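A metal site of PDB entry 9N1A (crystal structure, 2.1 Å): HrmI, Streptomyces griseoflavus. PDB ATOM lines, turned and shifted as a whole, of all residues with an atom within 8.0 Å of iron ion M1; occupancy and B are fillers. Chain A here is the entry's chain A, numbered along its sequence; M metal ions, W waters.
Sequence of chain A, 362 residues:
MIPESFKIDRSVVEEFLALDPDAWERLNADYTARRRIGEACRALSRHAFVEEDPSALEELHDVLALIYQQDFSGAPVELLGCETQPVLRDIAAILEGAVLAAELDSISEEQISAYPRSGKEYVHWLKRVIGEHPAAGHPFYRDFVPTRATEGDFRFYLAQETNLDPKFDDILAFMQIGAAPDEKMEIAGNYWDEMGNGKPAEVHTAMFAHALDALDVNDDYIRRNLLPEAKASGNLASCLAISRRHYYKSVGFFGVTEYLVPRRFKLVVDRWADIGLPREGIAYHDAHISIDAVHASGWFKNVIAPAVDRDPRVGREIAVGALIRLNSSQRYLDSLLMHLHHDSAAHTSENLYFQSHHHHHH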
ATOM      1  N   PHE A 168       4.534 -22.761 -25.861  1.00  0.00           N
ATOM      2  CA  PHE A 168       5.658 -23.027 -24.963  1.00  0.00           C
ATOM      3  C   PHE A 168       5.193 -23.316 -23.544  1.00  0.00           C
ATOM      4  O   PHE A 168       5.753 -24.189 -22.874  1.00  0.00           O
ATOM      5  CB  PHE A 168       6.618 -21.829 -24.914  1.00  0.00           C
ATOM      6  CG  PHE A 168       7.718 -21.881 -25.896  1.00  0.00           C
ATOM      7  CD1 PHE A 168       7.930 -22.994 -26.679  1.00  0.00           C
ATOM      8  CD2 PHE A 168       8.542 -20.773 -26.078  1.00  0.00           C
ATOM      9  CE1 PHE A 168       8.971 -23.013 -27.603  1.00  0.00           C
ATOM     10  CE2 PHE A 168       9.561 -20.770 -27.005  1.00  0.00           C
ATOM     11  CZ  PHE A 168       9.779 -21.895 -27.772  1.00  0.00           C
ATOM     12  N   LEU A 172       6.161 -26.805 -21.691  1.00  0.00           N
ATOM     13  CA  LEU A 172       6.882 -26.865 -20.423  1.00  0.00           C
ATOM     14  C   LEU A 172       6.078 -27.613 -19.379  1.00  0.00           C
ATOM     15  O   LEU A 172       6.632 -28.410 -18.610  1.00  0.00           O
ATOM     16  CB  LEU A 172       7.208 -25.451 -19.932  1.00  0.00           C
ATOM     17  CG  LEU A 172       8.286 -24.679 -20.738  1.00  0.00           C
ATOM     18  CD1 LEU A 172       8.219 -23.199 -20.480  1.00  0.00           C
ATOM     19  CD2 LEU A 172       9.684 -25.200 -20.410  1.00  0.00           C
ATOM     20  N   ASN A 190      10.629 -21.378 -15.349  1.00  0.00           N
ATOM     21  CA  ASN A 190      10.460 -21.014 -16.744  1.00  0.00           C
ATOM     22  C   ASN A 190       8.971 -20.891 -17.095  1.00  0.00           C
ATOM     23  O   ASN A 190       8.551 -19.892 -17.692  1.00  0.00           O
ATOM     24  CB  ASN A 190      11.152 -22.066 -17.617  1.00  0.00           C
ATOM     25  CG  ASN A 190      11.357 -21.629 -19.044  1.00  0.00           C
ATOM     26  OD1 ASN A 190      10.468 -21.020 -19.659  1.00  0.00           O
ATOM     27  ND2 ASN A 190      12.528 -21.950 -19.604  1.00  0.00           N
ATOM     28  N   TYR A 191       8.164 -21.883 -16.716  1.00  0.00           N
ATOM     29  CA  TYR A 191       6.719 -21.823 -16.973  1.00  0.00           C
ATOM     30  C   TYR A 191       6.090 -20.562 -16.366  1.00  0.00           C
ATOM     31  O   TYR A 191       5.309 -19.852 -17.007  1.00  0.00           O
ATOM     32  CB  TYR A 191       6.037 -23.084 -16.437  1.00  0.00           C
ATOM     33  CG  TYR A 191       4.503 -23.012 -16.331  1.00  0.00           C
ATOM     34  CD1 TYR A 191       3.700 -23.348 -17.417  1.00  0.00           C
ATOM     35  CD2 TYR A 191       3.886 -22.644 -15.143  1.00  0.00           C
ATOM     36  CE1 TYR A 191       2.308 -23.304 -17.328  1.00  0.00           C
ATOM     37  CE2 TYR A 191       2.469 -22.575 -15.041  1.00  0.00           C
ATOM     38  CZ  TYR A 191       1.701 -22.909 -16.150  1.00  0.00           C
ATOM     39  OH  TYR A 191       0.322 -22.869 -16.082  1.00  0.00           O
ATOM     40  N   ASP A 193       7.488 -17.728 -15.711  1.00  0.00           N
ATOM     41  CA  ASP A 193       7.824 -16.602 -16.583  1.00  0.00           C
ATOM     42  C   ASP A 193       6.926 -16.569 -17.825  1.00  0.00           C
ATOM     43  O   ASP A 193       6.493 -15.497 -18.258  1.00  0.00           O
ATOM     44  CB  ASP A 193       9.299 -16.673 -17.044  1.00  0.00           C
ATOM     45  CG  ASP A 193      10.308 -16.438 -15.935  1.00  0.00           C
ATOM     46  OD1 ASP A 193       9.985 -15.797 -14.914  1.00  0.00           O
ATOM     47  OD2 ASP A 193      11.458 -16.891 -16.121  1.00  0.00           O
ATOM     48  N   GLU A 194       6.666 -17.725 -18.429  1.00  0.00           N
ATOM     49  CA  GLU A 194       5.779 -17.766 -19.601  1.00  0.00           C
ATOM     50  C   GLU A 194       4.394 -17.224 -19.269  1.00  0.00           C
ATOM     51  O   GLU A 194       3.691 -16.711 -20.149  1.00  0.00           O
ATOM     52  CB  GLU A 194       5.660 -19.201 -20.139  1.00  0.00           C
ATOM     53  CG  GLU A 194       6.869 -19.712 -20.908  1.00  0.00           C
ATOM     54  CD  GLU A 194       7.032 -19.062 -22.276  1.00  0.00           C
ATOM     55  OE1 GLU A 194       6.002 -18.766 -22.924  1.00  0.00           O
ATOM     56  OE2 GLU A 194       8.197 -18.845 -22.687  1.00  0.00           O
ATOM     57  N   HIS A 204       3.538 -14.655 -22.192  1.00  0.00           N
ATOM     58  CA  HIS A 204       4.337 -14.625 -23.426  1.00  0.00           C
ATOM     59  C   HIS A 204       3.483 -14.892 -24.650  1.00  0.00           C
ATOM     60  O   HIS A 204       3.689 -14.263 -25.698  1.00  0.00           O
ATOM     61  CB  HIS A 204       5.487 -15.627 -23.351  1.00  0.00           C
ATOM     62  CG  HIS A 204       6.534 -15.236 -22.372  1.00  0.00           C
ATOM     63  ND1 HIS A 204       7.734 -15.914 -22.251  1.00  0.00           N
ATOM     64  CD2 HIS A 204       6.555 -14.252 -21.440  1.00  0.00           C
ATOM     65  CE1 HIS A 204       8.455 -15.348 -21.287  1.00  0.00           C
ATOM     66  NE2 HIS A 204       7.759 -14.342 -20.786  1.00  0.00           N
ATOM     67  N   PHE A 254      14.228 -28.452 -26.428  1.00  0.00           N
ATOM     68  CA  PHE A 254      13.898 -27.106 -25.987  1.00  0.00           C
ATOM     69  C   PHE A 254      15.100 -26.396 -25.364  1.00  0.00           C
ATOM     70  O   PHE A 254      15.135 -25.165 -25.355  1.00  0.00           O
ATOM     71  CB  PHE A 254      12.651 -27.209 -25.086  1.00  0.00           C
ATOM     72  CG  PHE A 254      11.462 -27.884 -25.791  1.00  0.00           C
ATOM     73  CD1 PHE A 254      10.769 -27.227 -26.787  1.00  0.00           C
ATOM     74  CD2 PHE A 254      11.112 -29.193 -25.519  1.00  0.00           C
ATOM     75  CE1 PHE A 254       9.732 -27.833 -27.452  1.00  0.00           C
ATOM     76  CE2 PHE A 254      10.067 -29.824 -26.200  1.00  0.00           C
ATOM     77  CZ  PHE A 254       9.378 -29.139 -27.164  1.00  0.00           C
ATOM     78  N   THR A 257      16.454 -24.659 -28.235  1.00  0.00           N
ATOM     79  CA  THR A 257      15.510 -23.591 -28.589  1.00  0.00           C
ATOM     80  C   THR A 257      15.798 -22.303 -27.817  1.00  0.00           C
ATOM     81  O   THR A 257      15.925 -21.237 -28.418  1.00  0.00           O
ATOM     82  CB  THR A 257      14.092 -24.065 -28.312  1.00  0.00           C
ATOM     83  OG1 THR A 257      13.729 -25.101 -29.244  1.00  0.00           O
ATOM     84  CG2 THR A 257      13.120 -22.914 -28.411  1.00  0.00           C
ATOM     85  N   GLU A 258      15.894 -22.382 -26.481  1.00  0.00           N
ATOM     86  CA  GLU A 258      16.174 -21.183 -25.683  1.00  0.00           C
ATOM     87  C   GLU A 258      17.533 -20.597 -26.024  1.00  0.00           C
ATOM     88  O   GLU A 258      17.705 -19.371 -26.103  1.00  0.00           O
ATOM     89  CB  GLU A 258      16.132 -21.493 -24.177  1.00  0.00           C
ATOM     90  CG  GLU A 258      14.901 -22.250 -23.696  1.00  0.00           C
ATOM     91  CD  GLU A 258      13.695 -21.346 -23.645  1.00  0.00           C
ATOM     92  OE1 GLU A 258      13.199 -20.976 -24.729  1.00  0.00           O
ATOM     93  OE2 GLU A 258      13.263 -20.996 -22.532  1.00  0.00           O
ATOM     94  N   TYR A 259      18.520 -21.474 -26.190  1.00  0.00           N
ATOM     95  CA  TYR A 259      19.903 -21.046 -26.412  1.00  0.00           C
ATOM     96  C   TYR A 259      20.027 -20.172 -27.662  1.00  0.00           C
ATOM     97  O   TYR A 259      20.783 -19.194 -27.660  1.00  0.00           O
ATOM     98  CB  TYR A 259      20.769 -22.299 -26.522  1.00  0.00           C
ATOM     99  CG  TYR A 259      22.259 -22.071 -26.645  1.00  0.00           C
ATOM    100  CD1 TYR A 259      22.958 -21.341 -25.694  1.00  0.00           C
ATOM    101  CD2 TYR A 259      22.959 -22.615 -27.721  1.00  0.00           C
ATOM    102  CE1 TYR A 259      24.348 -21.154 -25.814  1.00  0.00           C
ATOM    103  CE2 TYR A 259      24.320 -22.430 -27.860  1.00  0.00           C
ATOM    104  CZ  TYR A 259      25.009 -21.713 -26.902  1.00  0.00           C
ATOM    105  OH  TYR A 259      26.365 -21.556 -27.073  1.00  0.00           O
ATOM    106  N   VAL A 261      17.606 -18.359 -29.199  1.00  0.00           N
ATOM    107  CA  VAL A 261      16.665 -17.238 -29.346  1.00  0.00           C
ATOM    108  C   VAL A 261      17.364 -15.878 -29.308  1.00  0.00           C
ATOM    109  O   VAL A 261      17.094 -15.050 -30.187  1.00  0.00           O
ATOM    110  CB  VAL A 261      15.542 -17.353 -28.300  1.00  0.00           C
ATOM    111  CG1 VAL A 261      14.964 -15.971 -27.970  1.00  0.00           C
ATOM    112  CG2 VAL A 261      14.444 -18.285 -28.828  1.00  0.00           C
ATOM    113  N   TYR A 284       7.335  -8.845 -27.782  1.00  0.00           N
ATOM    114  CA  TYR A 284       7.659 -10.235 -27.489  1.00  0.00           C
ATOM    115  C   TYR A 284       9.129 -10.526 -27.777  1.00  0.00           C
ATOM    116  O   TYR A 284       9.878 -10.977 -26.904  1.00  0.00           O
ATOM    117  CB  TYR A 284       6.754 -11.177 -28.284  1.00  0.00           C
ATOM    118  CG  TYR A 284       7.135 -12.651 -28.202  1.00  0.00           C
ATOM    119  CD1 TYR A 284       6.638 -13.456 -27.162  1.00  0.00           C
ATOM    120  CD2 TYR A 284       8.000 -13.235 -29.131  1.00  0.00           C
ATOM    121  CE1 TYR A 284       6.995 -14.797 -27.063  1.00  0.00           C
ATOM    122  CE2 TYR A 284       8.349 -14.587 -29.049  1.00  0.00           C
ATOM    123  CZ  TYR A 284       7.841 -15.357 -28.019  1.00  0.00           C
ATOM    124  OH  TYR A 284       8.177 -16.690 -27.919  1.00  0.00           O
ATOM    125  N   HIS A 288      12.252 -11.256 -25.127  1.00  0.00           N
ATOM    126  CA  HIS A 288      12.894 -12.561 -25.109  1.00  0.00           C
ATOM    127  C   HIS A 288      14.399 -12.504 -25.341  1.00  0.00           C
ATOM    128  O   HIS A 288      15.085 -13.469 -25.004  1.00  0.00           O
ATOM    129  CB  HIS A 288      12.223 -13.477 -26.133  1.00  0.00           C
ATOM    130  CG  HIS A 288      11.034 -14.169 -25.565  1.00  0.00           C
ATOM    131  ND1 HIS A 288       9.912 -13.487 -25.151  1.00  0.00           N
ATOM    132  CD2 HIS A 288      10.827 -15.475 -25.262  1.00  0.00           C
ATOM    133  CE1 HIS A 288       9.040 -14.340 -24.644  1.00  0.00           C
ATOM    134  NE2 HIS A 288       9.575 -15.561 -24.696  1.00  0.00           N
ATOM    135  N   ILE A 291      15.254 -12.426 -21.716  1.00  0.00           N
ATOM    136  CA  ILE A 291      14.625 -13.511 -20.960  1.00  0.00           C
ATOM    137  C   ILE A 291      15.260 -14.842 -21.323  1.00  0.00           C
ATOM    138  O   ILE A 291      15.621 -15.643 -20.441  1.00  0.00           O
ATOM    139  CB  ILE A 291      13.098 -13.543 -21.182  1.00  0.00           C
ATOM    140  CG1 ILE A 291      12.391 -12.470 -20.353  1.00  0.00           C
ATOM    141  CG2 ILE A 291      12.535 -14.888 -20.813  1.00  0.00           C
ATOM    142  CD1 ILE A 291      11.303 -11.705 -21.121  1.00  0.00           C
ATOM    143  N   ASP A 292      15.423 -15.112 -22.608  1.00  0.00           N
ATOM    144  CA  ASP A 292      15.902 -16.428 -22.985  1.00  0.00           C
ATOM    145  C   ASP A 292      17.408 -16.586 -22.822  1.00  0.00           C
ATOM    146  O   ASP A 292      17.876 -17.726 -22.790  1.00  0.00           O
ATOM    147  CB  ASP A 292      15.433 -16.765 -24.393  1.00  0.00           C
ATOM    148  CG  ASP A 292      14.026 -17.333 -24.384  1.00  0.00           C
ATOM    149  OD1 ASP A 292      13.547 -17.652 -23.282  1.00  0.00           O
ATOM    150  OD2 ASP A 292      13.409 -17.469 -25.460  1.00  0.00           O
ATOM    151  N   ALA A 293      18.150 -15.487 -22.671  1.00  0.00           N
ATOM    152  CA  ALA A 293      19.520 -15.621 -22.157  1.00  0.00           C
ATOM    153  C   ALA A 293      19.519 -16.217 -20.751  1.00  0.00           C
ATOM    154  O   ALA A 293      20.343 -17.078 -20.421  1.00  0.00           O
ATOM    155  CB  ALA A 293      20.200 -14.248 -22.168  1.00  0.00           C
ATOM    156  N   VAL A 294      18.572 -15.769 -19.911  1.00  0.00           N
ATOM    157  CA  VAL A 294      18.453 -16.323 -18.563  1.00  0.00           C
ATOM    158  C   VAL A 294      17.826 -17.720 -18.602  1.00  0.00           C
ATOM    159  O   VAL A 294      18.257 -18.622 -17.871  1.00  0.00           O
ATOM    160  CB  VAL A 294      17.645 -15.357 -17.664  1.00  0.00           C
ATOM    161  CG1 VAL A 294      17.261 -16.003 -16.334  1.00  0.00           C
ATOM    162  CG2 VAL A 294      18.447 -14.079 -17.437  1.00  0.00           C
ATOM    163  N   HIS A 295      16.815 -17.930 -19.457  1.00  0.00           N
ATOM    164  CA  HIS A 295      16.235 -19.265 -19.581  1.00  0.00           C
ATOM    165  C   HIS A 295      17.277 -20.273 -20.059  1.00  0.00           C
ATOM    166  O   HIS A 295      17.363 -21.382 -19.511  1.00  0.00           O
ATOM    167  CB  HIS A 295      15.034 -19.251 -20.528  1.00  0.00           C
ATOM    168  CG  HIS A 295      13.797 -18.689 -19.919  1.00  0.00           C
ATOM    169  ND1 HIS A 295      12.620 -18.538 -20.627  1.00  0.00           N
ATOM    170  CD2 HIS A 295      13.540 -18.230 -18.667  1.00  0.00           C
ATOM    171  CE1 HIS A 295      11.700 -18.015 -19.843  1.00  0.00           C
ATOM    172  NE2 HIS A 295      12.231 -17.812 -18.649  1.00  0.00           N
ATOM    173  N   ALA A 296      18.069 -19.914 -21.068  1.00  0.00           N
ATOM    174  CA  ALA A 296      19.063 -20.859 -21.599  1.00  0.00           C
ATOM    175  C   ALA A 296      20.101 -21.204 -20.549  1.00  0.00           C
ATOM    176  O   ALA A 296      20.501 -22.373 -20.412  1.00  0.00           O
ATOM    177  CB  ALA A 296      19.753 -20.274 -22.831  1.00  0.00           C
ATOM    178  N   TRP A 299      18.572 -23.473 -18.007  1.00  0.00           N
ATOM    179  CA  TRP A 299      18.275 -24.782 -18.584  1.00  0.00           C
ATOM    180  C   TRP A 299      19.514 -25.672 -18.637  1.00  0.00           C
ATOM    181  O   TRP A 299      19.460 -26.856 -18.281  1.00  0.00           O
ATOM    182  CB  TRP A 299      17.676 -24.582 -19.984  1.00  0.00           C
ATOM    183  CG  TRP A 299      16.959 -25.776 -20.449  1.00  0.00           C
ATOM    184  CD1 TRP A 299      17.499 -26.836 -21.108  1.00  0.00           C
ATOM    185  CD2 TRP A 299      15.569 -26.069 -20.278  1.00  0.00           C
ATOM    186  NE1 TRP A 299      16.534 -27.778 -21.363  1.00  0.00           N
ATOM    187  CE2 TRP A 299      15.336 -27.332 -20.868  1.00  0.00           C
ATOM    188  CE3 TRP A 299      14.494 -25.387 -19.698  1.00  0.00           C
ATOM    189  CZ2 TRP A 299      14.066 -27.929 -20.889  1.00  0.00           C
ATOM    190  CZ3 TRP A 299      13.233 -25.985 -19.723  1.00  0.00           C
ATOM    191  CH2 TRP A 299      13.034 -27.234 -20.314  1.00  0.00           C
HETATM  192 FE    FE M   1      12.023 -18.913 -22.682  1.00  0.00          FE
HETATM  193 FE    FE M   2       8.885 -17.203 -23.614  1.00  0.00          FE
HETATM  194  O   HOH W   1      11.419 -19.243 -24.843  1.00  0.00           O
HETATM  195  O   HOH W   2      10.426 -20.195 -22.124  1.00  0.00           O
HETATM  196  O   HOH W   3      10.764 -17.327 -22.603  1.00  0.00           O
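Residues that only touch iron ion M1: Asn 190 (3.9995 Å) and Glu 194 (3.8 Å).
Of the 21 residues printed, 5 come within 4 Å of iron ion M1.
The nearest printed residue that does not touch iron ion M1 is His 288 (4.5 Å).
Iron ion M1 is bound by water W3 (2.0 Å), the side-chain carboxylate of Asp 292 (2.1 Å), water W2 (2.1 Å), a ring nitrogen (ND1) of His 295 (2.2 Å), water W1 (2.3 Å) and the side-chain carboxylate of Glu 258 (2.4 Å).
ND1 of His 295 lies close to OD1 of Asn 190 (3.4 Å).
NE2 of His 295 sits at hydrogen-bond distance from OD2 of Asp 193, at 2.8 Å.
The side-chain amide nitrogen of Asn 190 lies close to the side-chain carboxylate of Glu 258, at 3.2 Å.
Water W1 lies within hydrogen-bond range of the side-chain carboxylate of Glu 258 and the side-chain carboxylate of Asp 292.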
